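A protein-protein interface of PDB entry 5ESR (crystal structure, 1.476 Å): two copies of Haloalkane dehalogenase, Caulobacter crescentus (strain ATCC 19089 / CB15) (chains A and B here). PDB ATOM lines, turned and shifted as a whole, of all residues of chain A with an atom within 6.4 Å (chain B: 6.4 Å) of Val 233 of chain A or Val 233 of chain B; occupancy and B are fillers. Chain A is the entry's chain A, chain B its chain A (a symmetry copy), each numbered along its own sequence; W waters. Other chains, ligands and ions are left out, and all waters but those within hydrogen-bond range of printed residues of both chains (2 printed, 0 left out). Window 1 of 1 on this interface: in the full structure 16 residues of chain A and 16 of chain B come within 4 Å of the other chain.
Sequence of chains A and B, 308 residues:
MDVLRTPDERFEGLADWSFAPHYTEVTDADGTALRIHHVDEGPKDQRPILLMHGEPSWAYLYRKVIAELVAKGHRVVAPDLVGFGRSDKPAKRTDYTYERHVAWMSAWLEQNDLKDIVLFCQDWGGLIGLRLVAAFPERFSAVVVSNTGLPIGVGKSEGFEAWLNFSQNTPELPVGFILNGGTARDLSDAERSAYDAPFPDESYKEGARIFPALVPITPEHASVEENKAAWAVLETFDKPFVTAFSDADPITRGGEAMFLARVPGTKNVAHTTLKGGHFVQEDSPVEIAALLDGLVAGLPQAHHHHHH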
ATOM      1  N   VAL A 133     -12.329   1.693  30.920  1.00  0.00           N
ATOM      2  CA  VAL A 133     -12.529   1.023  29.634  1.00  0.00           C
ATOM      3  C   VAL A 133     -13.859   1.470  29.042  1.00  0.00           C
ATOM      4  O   VAL A 133     -13.929   1.783  27.859  1.00  0.00           O
ATOM      5  CB  VAL A 133     -12.500  -0.507  29.783  1.00  0.00           C
ATOM      6  CG1 VAL A 133     -12.820  -1.188  28.466  1.00  0.00           C
ATOM      7  CG2 VAL A 133     -11.134  -0.968  30.310  1.00  0.00           C
ATOM      8  N   ALA A 134     -14.913   1.534  29.848  1.00  0.00           N
ATOM      9  CA  ALA A 134     -16.221   1.936  29.332  1.00  0.00           C
ATOM     10  C   ALA A 134     -16.280   3.413  28.927  1.00  0.00           C
ATOM     11  O   ALA A 134     -17.033   3.769  28.027  1.00  0.00           O
ATOM     12  CB  ALA A 134     -17.311   1.627  30.364  1.00  0.00           C
ATOM     13  N   ALA A 135     -15.491   4.256  29.571  1.00  0.00           N
ATOM     14  CA  ALA A 135     -15.457   5.671  29.227  1.00  0.00           C
ATOM     15  C   ALA A 135     -14.587   5.953  28.016  1.00  0.00           C
ATOM     16  O   ALA A 135     -14.893   6.850  27.240  1.00  0.00           O
ATOM     17  CB  ALA A 135     -14.959   6.488  30.398  1.00  0.00           C
ATOM     18  N   PRO A 137     -13.040   3.410  25.568  1.00  0.00           N
ATOM     19  CA  PRO A 137     -12.724   2.048  25.117  1.00  0.00           C
ATOM     20  C   PRO A 137     -11.626   2.000  24.054  1.00  0.00           C
ATOM     21  O   PRO A 137     -10.873   1.038  24.000  1.00  0.00           O
ATOM     22  CB  PRO A 137     -14.057   1.541  24.568  1.00  0.00           C
ATOM     23  CG  PRO A 137     -14.851   2.771  24.279  1.00  0.00           C
ATOM     24  CD  PRO A 137     -14.451   3.751  25.340  1.00  0.00           C
ATOM     25  N   LYS A 228     -24.388   0.169  35.407  1.00  0.00           N
ATOM     26  CA  LYS A 228     -25.266  -0.446  34.421  1.00  0.00           C
ATOM     27  C   LYS A 228     -25.008   0.161  33.056  1.00  0.00           C
ATOM     28  O   LYS A 228     -24.964  -0.542  32.045  1.00  0.00           O
ATOM     29  CB  LYS A 228     -26.734  -0.292  34.818  1.00  0.00           C
ATOM     30  CG  LYS A 228     -27.154  -1.157  35.999  1.00  0.00           C
ATOM     31  CD  LYS A 228     -28.627  -0.935  36.346  1.00  0.00           C
ATOM     32  CE  LYS A 228     -29.086  -1.841  37.464  1.00  0.00           C
ATOM     33  NZ  LYS A 228     -30.533  -1.608  37.780  1.00  0.00           N
ATOM     34  N   ALA A 229     -24.811   1.468  33.012  1.00  0.00           N
ATOM     35  CA  ALA A 229     -24.504   2.112  31.745  1.00  0.00           C
ATOM     36  C   ALA A 229     -23.163   1.640  31.170  1.00  0.00           C
ATOM     37  O   ALA A 229     -23.033   1.375  29.968  1.00  0.00           O
ATOM     38  CB  ALA A 229     -24.519   3.610  31.917  1.00  0.00           C
ATOM     39  N   ALA A 230     -22.156   1.522  32.024  1.00  0.00           N
ATOM     40  CA  ALA A 230     -20.856   1.055  31.597  1.00  0.00           C
ATOM     41  C   ALA A 230     -20.939  -0.349  30.999  1.00  0.00           C
ATOM     42  O   ALA A 230     -20.228  -0.655  30.033  1.00  0.00           O
ATOM     43  CB  ALA A 230     -19.869   1.081  32.751  1.00  0.00           C
ATOM     44  N   TRP A 231     -21.782  -1.206  31.570  1.00  0.00           N
ATOM     45  CA  TRP A 231     -21.964  -2.546  31.021  1.00  0.00           C
ATOM     46  C   TRP A 231     -22.461  -2.496  29.582  1.00  0.00           C
ATOM     47  O   TRP A 231     -22.102  -3.354  28.801  1.00  0.00           O
ATOM     48  CB  TRP A 231     -22.917  -3.378  31.870  1.00  0.00           C
ATOM     49  CG  TRP A 231     -22.231  -4.131  32.960  1.00  0.00           C
ATOM     50  CD1 TRP A 231     -22.275  -3.859  34.308  1.00  0.00           C
ATOM     51  CD2 TRP A 231     -21.392  -5.287  32.814  1.00  0.00           C
ATOM     52  NE1 TRP A 231     -21.516  -4.769  34.996  1.00  0.00           N
ATOM     53  CE2 TRP A 231     -20.960  -5.656  34.108  1.00  0.00           C
ATOM     54  CE3 TRP A 231     -20.951  -6.036  31.714  1.00  0.00           C
ATOM     55  CZ2 TRP A 231     -20.116  -6.748  34.335  1.00  0.00           C
ATOM     56  CZ3 TRP A 231     -20.123  -7.119  31.942  1.00  0.00           C
ATOM     57  CH2 TRP A 231     -19.712  -7.467  33.237  1.00  0.00           C
ATOM     58  N   ALA A 232     -23.281  -1.507  29.222  1.00  0.00           N
ATOM     59  CA  ALA A 232     -23.723  -1.403  27.827  1.00  0.00           C
ATOM     60  C   ALA A 232     -22.551  -1.135  26.887  1.00  0.00           C
ATOM     61  O   ALA A 232     -22.550  -1.588  25.732  1.00  0.00           O
ATOM     62  CB  ALA A 232     -24.773  -0.337  27.667  1.00  0.00           C
ATOM     63  N   VAL A 233     -21.540  -0.404  27.357  1.00  0.00           N
ATOM     64  CA  VAL A 233     -20.338  -0.215  26.557  1.00  0.00           C
ATOM     65  C   VAL A 233     -19.543  -1.516  26.490  1.00  0.00           C
ATOM     66  O   VAL A 233     -19.067  -1.894  25.426  1.00  0.00           O
ATOM     67  CB  VAL A 233     -19.462   0.913  27.097  1.00  0.00           C
ATOM     68  CG1 VAL A 233     -18.270   1.144  26.165  1.00  0.00           C
ATOM     69  CG2 VAL A 233     -20.271   2.187  27.236  1.00  0.00           C
ATOM     70  N   LEU A 234     -19.379  -2.191  27.625  1.00  0.00           N
ATOM     71  CA  LEU A 234     -18.648  -3.449  27.626  1.00  0.00           C
ATOM     72  C   LEU A 234     -19.309  -4.507  26.744  1.00  0.00           C
ATOM     73  O   LEU A 234     -18.606  -5.369  26.196  1.00  0.00           O
ATOM     74  CB  LEU A 234     -18.456  -3.982  29.045  1.00  0.00           C
ATOM     75  CG  LEU A 234     -17.676  -3.082  29.995  1.00  0.00           C
ATOM     76  CD1 LEU A 234     -17.505  -3.794  31.334  1.00  0.00           C
ATOM     77  CD2 LEU A 234     -16.320  -2.656  29.401  1.00  0.00           C
ATOM     78  N   GLU A 235     -20.629  -4.445  26.575  1.00  0.00           N
ATOM     79  CA  GLU A 235     -21.347  -5.341  25.653  1.00  0.00           C
ATOM     80  C   GLU A 235     -20.930  -5.151  24.201  1.00  0.00           C
ATOM     81  O   GLU A 235     -21.259  -5.980  23.357  1.00  0.00           O
ATOM     82  CB  GLU A 235     -22.865  -5.207  25.790  1.00  0.00           C
ATOM     83  CG  GLU A 235     -23.338  -5.804  27.090  1.00  0.00           C
ATOM     84  CD  GLU A 235     -24.844  -5.905  27.195  1.00  0.00           C
ATOM     85  OE1 GLU A 235     -25.549  -5.189  26.462  1.00  0.00           O
ATOM     86  OE2 GLU A 235     -25.336  -6.725  27.987  1.00  0.00           O
ATOM     87  N   THR A 236     -20.239  -4.051  23.920  1.00  0.00           N
ATOM     88  CA  THR A 236     -19.719  -3.768  22.580  1.00  0.00           C
ATOM     89  C   THR A 236     -18.216  -3.966  22.470  1.00  0.00           C
ATOM     90  O   THR A 236     -17.659  -3.775  21.396  1.00  0.00           O
ATOM     91  CB  THR A 236     -20.034  -2.312  22.105  1.00  0.00           C
ATOM     92  OG1 THR A 236     -19.173  -1.360  22.754  1.00  0.00           O
ATOM     93  CG2 THR A 236     -21.487  -1.960  22.329  1.00  0.00           C
ATOM     94  N   PHE A 237     -17.560  -4.335  23.567  1.00  0.00           N
ATOM     95  CA  PHE A 237     -16.096  -4.387  23.610  1.00  0.00           C
ATOM     96  C   PHE A 237     -15.624  -5.733  23.079  1.00  0.00           C
ATOM     97  O   PHE A 237     -15.834  -6.758  23.701  1.00  0.00           O
ATOM     98  CB  PHE A 237     -15.567  -4.160  25.023  1.00  0.00           C
ATOM     99  CG  PHE A 237     -14.087  -3.957  25.079  1.00  0.00           C
ATOM    100  CD1 PHE A 237     -13.235  -5.048  25.195  1.00  0.00           C
ATOM    101  CD2 PHE A 237     -13.545  -2.690  24.978  1.00  0.00           C
ATOM    102  CE1 PHE A 237     -11.869  -4.876  25.238  1.00  0.00           C
ATOM    103  CE2 PHE A 237     -12.166  -2.509  25.005  1.00  0.00           C
ATOM    104  CZ  PHE A 237     -11.331  -3.605  25.147  1.00  0.00           C
ATOM    105  N   PRO A 264     -18.310  -9.386  24.321  1.00  0.00           N
ATOM    106  CA  PRO A 264     -17.954 -10.176  23.133  1.00  0.00           C
ATOM    107  C   PRO A 264     -16.478 -10.539  23.029  1.00  0.00           C
ATOM    108  O   PRO A 264     -16.157 -11.603  22.481  1.00  0.00           O
ATOM    109  CB  PRO A 264     -18.353  -9.274  21.964  1.00  0.00           C
ATOM    110  CG  PRO A 264     -19.153  -8.178  22.521  1.00  0.00           C
ATOM    111  CD  PRO A 264     -18.925  -8.087  23.975  1.00  0.00           C
ATOM    112  N   VAL B 133     -27.806   1.790  17.103  1.00  0.00           N
ATOM    113  CA  VAL B 133     -26.440   2.313  17.081  1.00  0.00           C
ATOM    114  C   VAL B 133     -25.746   1.946  18.385  1.00  0.00           C
ATOM    115  O   VAL B 133     -24.605   1.499  18.368  1.00  0.00           O
ATOM    116  CB  VAL B 133     -26.421   3.837  16.879  1.00  0.00           C
ATOM    117  CG1 VAL B 133     -25.008   4.380  16.970  1.00  0.00           C
ATOM    118  CG2 VAL B 133     -27.054   4.206  15.529  1.00  0.00           C
ATOM    119  N   ALA B 134     -26.421   2.099  19.519  1.00  0.00           N
ATOM    120  CA  ALA B 134     -25.799   1.783  20.804  1.00  0.00           C
ATOM    121  C   ALA B 134     -25.556   0.284  21.003  1.00  0.00           C
ATOM    122  O   ALA B 134     -24.617  -0.096  21.694  1.00  0.00           O
ATOM    123  CB  ALA B 134     -26.653   2.337  21.951  1.00  0.00           C
ATOM    124  N   ALA B 135     -26.380  -0.555  20.398  1.00  0.00           N
ATOM    125  CA  ALA B 135     -26.201  -1.997  20.503  1.00  0.00           C
ATOM    126  C   ALA B 135     -25.142  -2.522  19.552  1.00  0.00           C
ATOM    127  O   ALA B 135     -24.438  -3.468  19.881  1.00  0.00           O
ATOM    128  CB  ALA B 135     -27.507  -2.713  20.237  1.00  0.00           C
ATOM    129  N   PRO B 137     -22.631  -0.488  17.450  1.00  0.00           N
ATOM    130  CA  PRO B 137     -22.073   0.764  16.921  1.00  0.00           C
ATOM    131  C   PRO B 137     -21.151   0.558  15.720  1.00  0.00           C
ATOM    132  O   PRO B 137     -21.081   1.416  14.852  1.00  0.00           O
ATOM    133  CB  PRO B 137     -21.315   1.344  18.115  1.00  0.00           C
ATOM    134  CG  PRO B 137     -21.072   0.182  19.021  1.00  0.00           C
ATOM    135  CD  PRO B 137     -22.274  -0.697  18.860  1.00  0.00           C
ATOM    136  N   LYS B 228     -30.619   5.183  29.288  1.00  0.00           N
ATOM    137  CA  LYS B 228     -29.472   5.764  29.973  1.00  0.00           C
ATOM    138  C   LYS B 228     -28.224   4.967  29.649  1.00  0.00           C
ATOM    139  O   LYS B 228     -27.154   5.531  29.411  1.00  0.00           O
ATOM    140  CB  LYS B 228     -29.705   5.823  31.482  1.00  0.00           C
ATOM    141  CG  LYS B 228     -30.724   6.869  31.915  1.00  0.00           C
ATOM    142  CD  LYS B 228     -30.914   6.857  33.433  1.00  0.00           C
ATOM    143  CE  LYS B 228     -31.862   7.939  33.892  1.00  0.00           C
ATOM    144  NZ  LYS B 228     -32.026   7.909  35.381  1.00  0.00           N
ATOM    145  N   ALA B 229     -28.348   3.652  29.612  1.00  0.00           N
ATOM    146  CA  ALA B 229     -27.207   2.825  29.254  1.00  0.00           C
ATOM    147  C   ALA B 229     -26.748   3.072  27.812  1.00  0.00           C
ATOM    148  O   ALA B 229     -25.548   3.169  27.523  1.00  0.00           O
ATOM    149  CB  ALA B 229     -27.540   1.372  29.473  1.00  0.00           C
ATOM    150  N   ALA B 230     -27.698   3.182  26.895  1.00  0.00           N
ATOM    151  CA  ALA B 230     -27.381   3.446  25.508  1.00  0.00           C
ATOM    152  C   ALA B 230     -26.625   4.765  25.353  1.00  0.00           C
ATOM    153  O   ALA B 230     -25.724   4.869  24.511  1.00  0.00           O
ATOM    154  CB  ALA B 230     -28.641   3.455  24.660  1.00  0.00           C
ATOM    155  N   TRP B 231     -26.993   5.775  26.139  1.00  0.00           N
ATOM    156  CA  TRP B 231     -26.281   7.048  26.094  1.00  0.00           C
ATOM    157  C   TRP B 231     -24.808   6.875  26.438  1.00  0.00           C
ATOM    158  O   TRP B 231     -23.985   7.585  25.895  1.00  0.00           O
ATOM    159  CB  TRP B 231     -26.913   8.080  27.022  1.00  0.00           C
ATOM    160  CG  TRP B 231     -27.987   8.881  26.366  1.00  0.00           C
ATOM    161  CD1 TRP B 231     -29.342   8.785  26.587  1.00  0.00           C
ATOM    162  CD2 TRP B 231     -27.816   9.910  25.380  1.00  0.00           C
ATOM    163  NE1 TRP B 231     -30.011   9.684  25.798  1.00  0.00           N
ATOM    164  CE2 TRP B 231     -29.104  10.386  25.046  1.00  0.00           C
ATOM    165  CE3 TRP B 231     -26.701  10.463  24.735  1.00  0.00           C
ATOM    166  CZ2 TRP B 231     -29.309  11.398  24.101  1.00  0.00           C
ATOM    167  CZ3 TRP B 231     -26.906  11.469  23.808  1.00  0.00           C
ATOM    168  CH2 TRP B 231     -28.193  11.926  23.497  1.00  0.00           C
ATOM    169  N   ALA B 232     -24.464   5.946  27.331  1.00  0.00           N
ATOM    170  CA  ALA B 232     -23.046   5.719  27.632  1.00  0.00           C
ATOM    171  C   ALA B 232     -22.288   5.209  26.410  1.00  0.00           C
ATOM    172  O   ALA B 232     -21.100   5.512  26.230  1.00  0.00           O
ATOM    173  CB  ALA B 232     -22.880   4.765  28.784  1.00  0.00           C
ATOM    174  N   VAL B 233     -22.954   4.435  25.553  1.00  0.00           N
ATOM    175  CA  VAL B 233     -22.330   4.016  24.305  1.00  0.00           C
ATOM    176  C   VAL B 233     -22.216   5.202  23.353  1.00  0.00           C
ATOM    177  O   VAL B 233     -21.181   5.391  22.723  1.00  0.00           O
ATOM    178  CB  VAL B 233     -23.093   2.874  23.638  1.00  0.00           C
ATOM    179  CG1 VAL B 233     -22.342   2.398  22.392  1.00  0.00           C
ATOM    180  CG2 VAL B 233     -23.273   1.724  24.609  1.00  0.00           C
ATOM    181  N   LEU B 234     -23.281   5.991  23.228  1.00  0.00           N
ATOM    182  CA  LEU B 234     -23.230   7.151  22.351  1.00  0.00           C
ATOM    183  C   LEU B 234     -22.163   8.158  22.778  1.00  0.00           C
ATOM    184  O   LEU B 234     -21.612   8.862  21.919  1.00  0.00           O
ATOM    185  CB  LEU B 234     -24.594   7.831  22.245  1.00  0.00           C
ATOM    186  CG  LEU B 234     -25.724   6.975  21.688  1.00  0.00           C
ATOM    187  CD1 LEU B 234     -26.987   7.824  21.573  1.00  0.00           C
ATOM    188  CD2 LEU B 234     -25.349   6.332  20.340  1.00  0.00           C
ATOM    189  N   GLU B 235     -21.845   8.222  24.070  1.00  0.00           N
ATOM    190  CA  GLU B 235     -20.751   9.070  24.569  1.00  0.00           C
ATOM    191  C   GLU B 235     -19.389   8.657  24.028  1.00  0.00           C
ATOM    192  O   GLU B 235     -18.425   9.406  24.160  1.00  0.00           O
ATOM    193  CB  GLU B 235     -20.718   9.123  26.098  1.00  0.00           C
ATOM    194  CG  GLU B 235     -21.878   9.925  26.629  1.00  0.00           C
ATOM    195  CD  GLU B 235     -21.790  10.204  28.113  1.00  0.00           C
ATOM    196  OE1 GLU B 235     -21.062   9.485  28.820  1.00  0.00           O
ATOM    197  OE2 GLU B 235     -22.422  11.166  28.581  1.00  0.00           O
ATOM    198  N   THR B 236     -19.316   7.461  23.453  1.00  0.00           N
ATOM    199  CA  THR B 236     -18.087   6.958  22.833  1.00  0.00           C
ATOM    200  C   THR B 236     -18.138   6.973  21.314  1.00  0.00           C
ATOM    201  O   THR B 236     -17.166   6.590  20.674  1.00  0.00           O
ATOM    202  CB  THR B 236     -17.742   5.498  23.273  1.00  0.00           C
ATOM    203  OG1 THR B 236     -18.591   4.545  22.611  1.00  0.00           O
ATOM    204  CG2 THR B 236     -17.828   5.340  24.774  1.00  0.00           C
ATOM    205  N   PHE B 237     -19.258   7.401  20.737  1.00  0.00           N
ATOM    206  CA  PHE B 237     -19.470   7.296  19.290  1.00  0.00           C
ATOM    207  C   PHE B 237     -18.854   8.505  18.602  1.00  0.00           C
ATOM    208  O   PHE B 237     -19.329   9.616  18.747  1.00  0.00           O
ATOM    209  CB  PHE B 237     -20.952   7.188  18.947  1.00  0.00           C
ATOM    210  CG  PHE B 237     -21.208   6.832  17.518  1.00  0.00           C
ATOM    211  CD1 PHE B 237     -21.304   7.828  16.554  1.00  0.00           C
ATOM    212  CD2 PHE B 237     -21.314   5.509  17.129  1.00  0.00           C
ATOM    213  CE1 PHE B 237     -21.529   7.512  15.232  1.00  0.00           C
ATOM    214  CE2 PHE B 237     -21.525   5.182  15.794  1.00  0.00           C
ATOM    215  CZ  PHE B 237     -21.645   6.188  14.850  1.00  0.00           C
ATOM    216  N   PRO B 264     -19.354  12.558  20.930  1.00  0.00           N
ATOM    217  CA  PRO B 264     -18.136  13.151  20.355  1.00  0.00           C
ATOM    218  C   PRO B 264     -18.171  13.332  18.843  1.00  0.00           C
ATOM    219  O   PRO B 264     -17.551  14.278  18.336  1.00  0.00           O
ATOM    220  CB  PRO B 264     -17.035  12.160  20.737  1.00  0.00           C
ATOM    221  CG  PRO B 264     -17.610  11.237  21.721  1.00  0.00           C
ATOM    222  CD  PRO B 264     -19.082  11.302  21.662  1.00  0.00           C
HETATM  223  O   HOH W   1     -24.811  -1.566  24.085  1.00  0.00           O
HETATM  224  O   HOH W   2     -19.206   5.537  28.289  1.00  0.00           O
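Pro 137 of chain A touches Thr 236 of chain B, and with the chains exchanged Thr 236 of chain A touches Pro 137 of chain B.
Ala 229 of chain A touches its own counterpart, Ala 229 of chain B.
Ala 232 of chain A touches Val 233 of chain B, and with the chains exchanged Val 233 of chain A touches Ala 232 of chain B.
Val 233 of chain B touches its own counterpart, Val 233 of chain A.
The side-chain hydroxyl (OG1) of Thr 236 of chain B sits at hydrogen-bond distance from the backbone carbonyl oxygen (O) of Val 233 of chain B.
O of Val 233 of chain A lies within hydrogen-bond range of OG1 of Thr 236 of chain A, 2.7 Å away.
Among the printed residues, merely in contact across the chains: Ala 134 of chain A with Thr 236 of chain B (3.7 Å), Pro 137 of chain A with Thr 236 of chain B (3.8 Å), Ala 229 of chain A with Ala 229 of chain B (3.7 Å), Ala 229 of chain A with Ala 232 of chain B (3.6 Å), Ala 232 of chain A with Ala 229 of chain B (3.6 Å), Ala 232 of chain A with Val 233 of chain B (3.6 Å), Val 233 of chain A with Ala 232 of chain B (3.6 Å), Val 233 of chain A with Val 233 of chain B (3.9 Å), Thr 236 of chain A with Ala 134 of chain B (3.7 Å) and Thr 236 of chain A with Pro 137 of chain B (3.8 Å).
Hydrophobic or aromatic side chains of chain A that line the printed part of chain B: Pro 137, Ala 229, Ala 232 and Val 233.
Of the 15 printed residues of chain B, 6 touch a printed residue of chain A.
Hydrophobic or aromatic side chains of chain B that line the printed part of chain A: Pro 137, Ala 229, Ala 232 and Val 233.
Along chain B the printed residues that touch a printed residue of chain A span positions 134 to 236.
Val 133 of chain A touches none of the printed residues of chain B.
Val 233 of chain A touches just these residues of chain B: Ala 232 (3.6 Å) and Val 233 (3.9 Å).
Of the printed residues of chain A, Pro 137 of chain B touches Thr 236 (3.8 Å).
Printed residues of chain A within 4 Å of Ala 229 of chain B: Ala 229 and Ala 232.
Of chain A, only Ala 232 and Val 233 come within 4 Å of Val 233 of chain B.
The nearest residue of chain A that does not touch Val 233 of chain B is Thr 236 of chain A (4.4 Å).
Water W2 lies within hydrogen-bond range of the backbone carbonyl oxygen of Ala 232 of chain B and the backbone carbonyl oxygen of Ala 134 of chain A.
Water W1 bridges the backbone carbonyl oxygen of Ala 232 of chain A (2.8 Å) and the backbone carbonyl oxygen of Ala 134 of chain B (2.8 Å).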
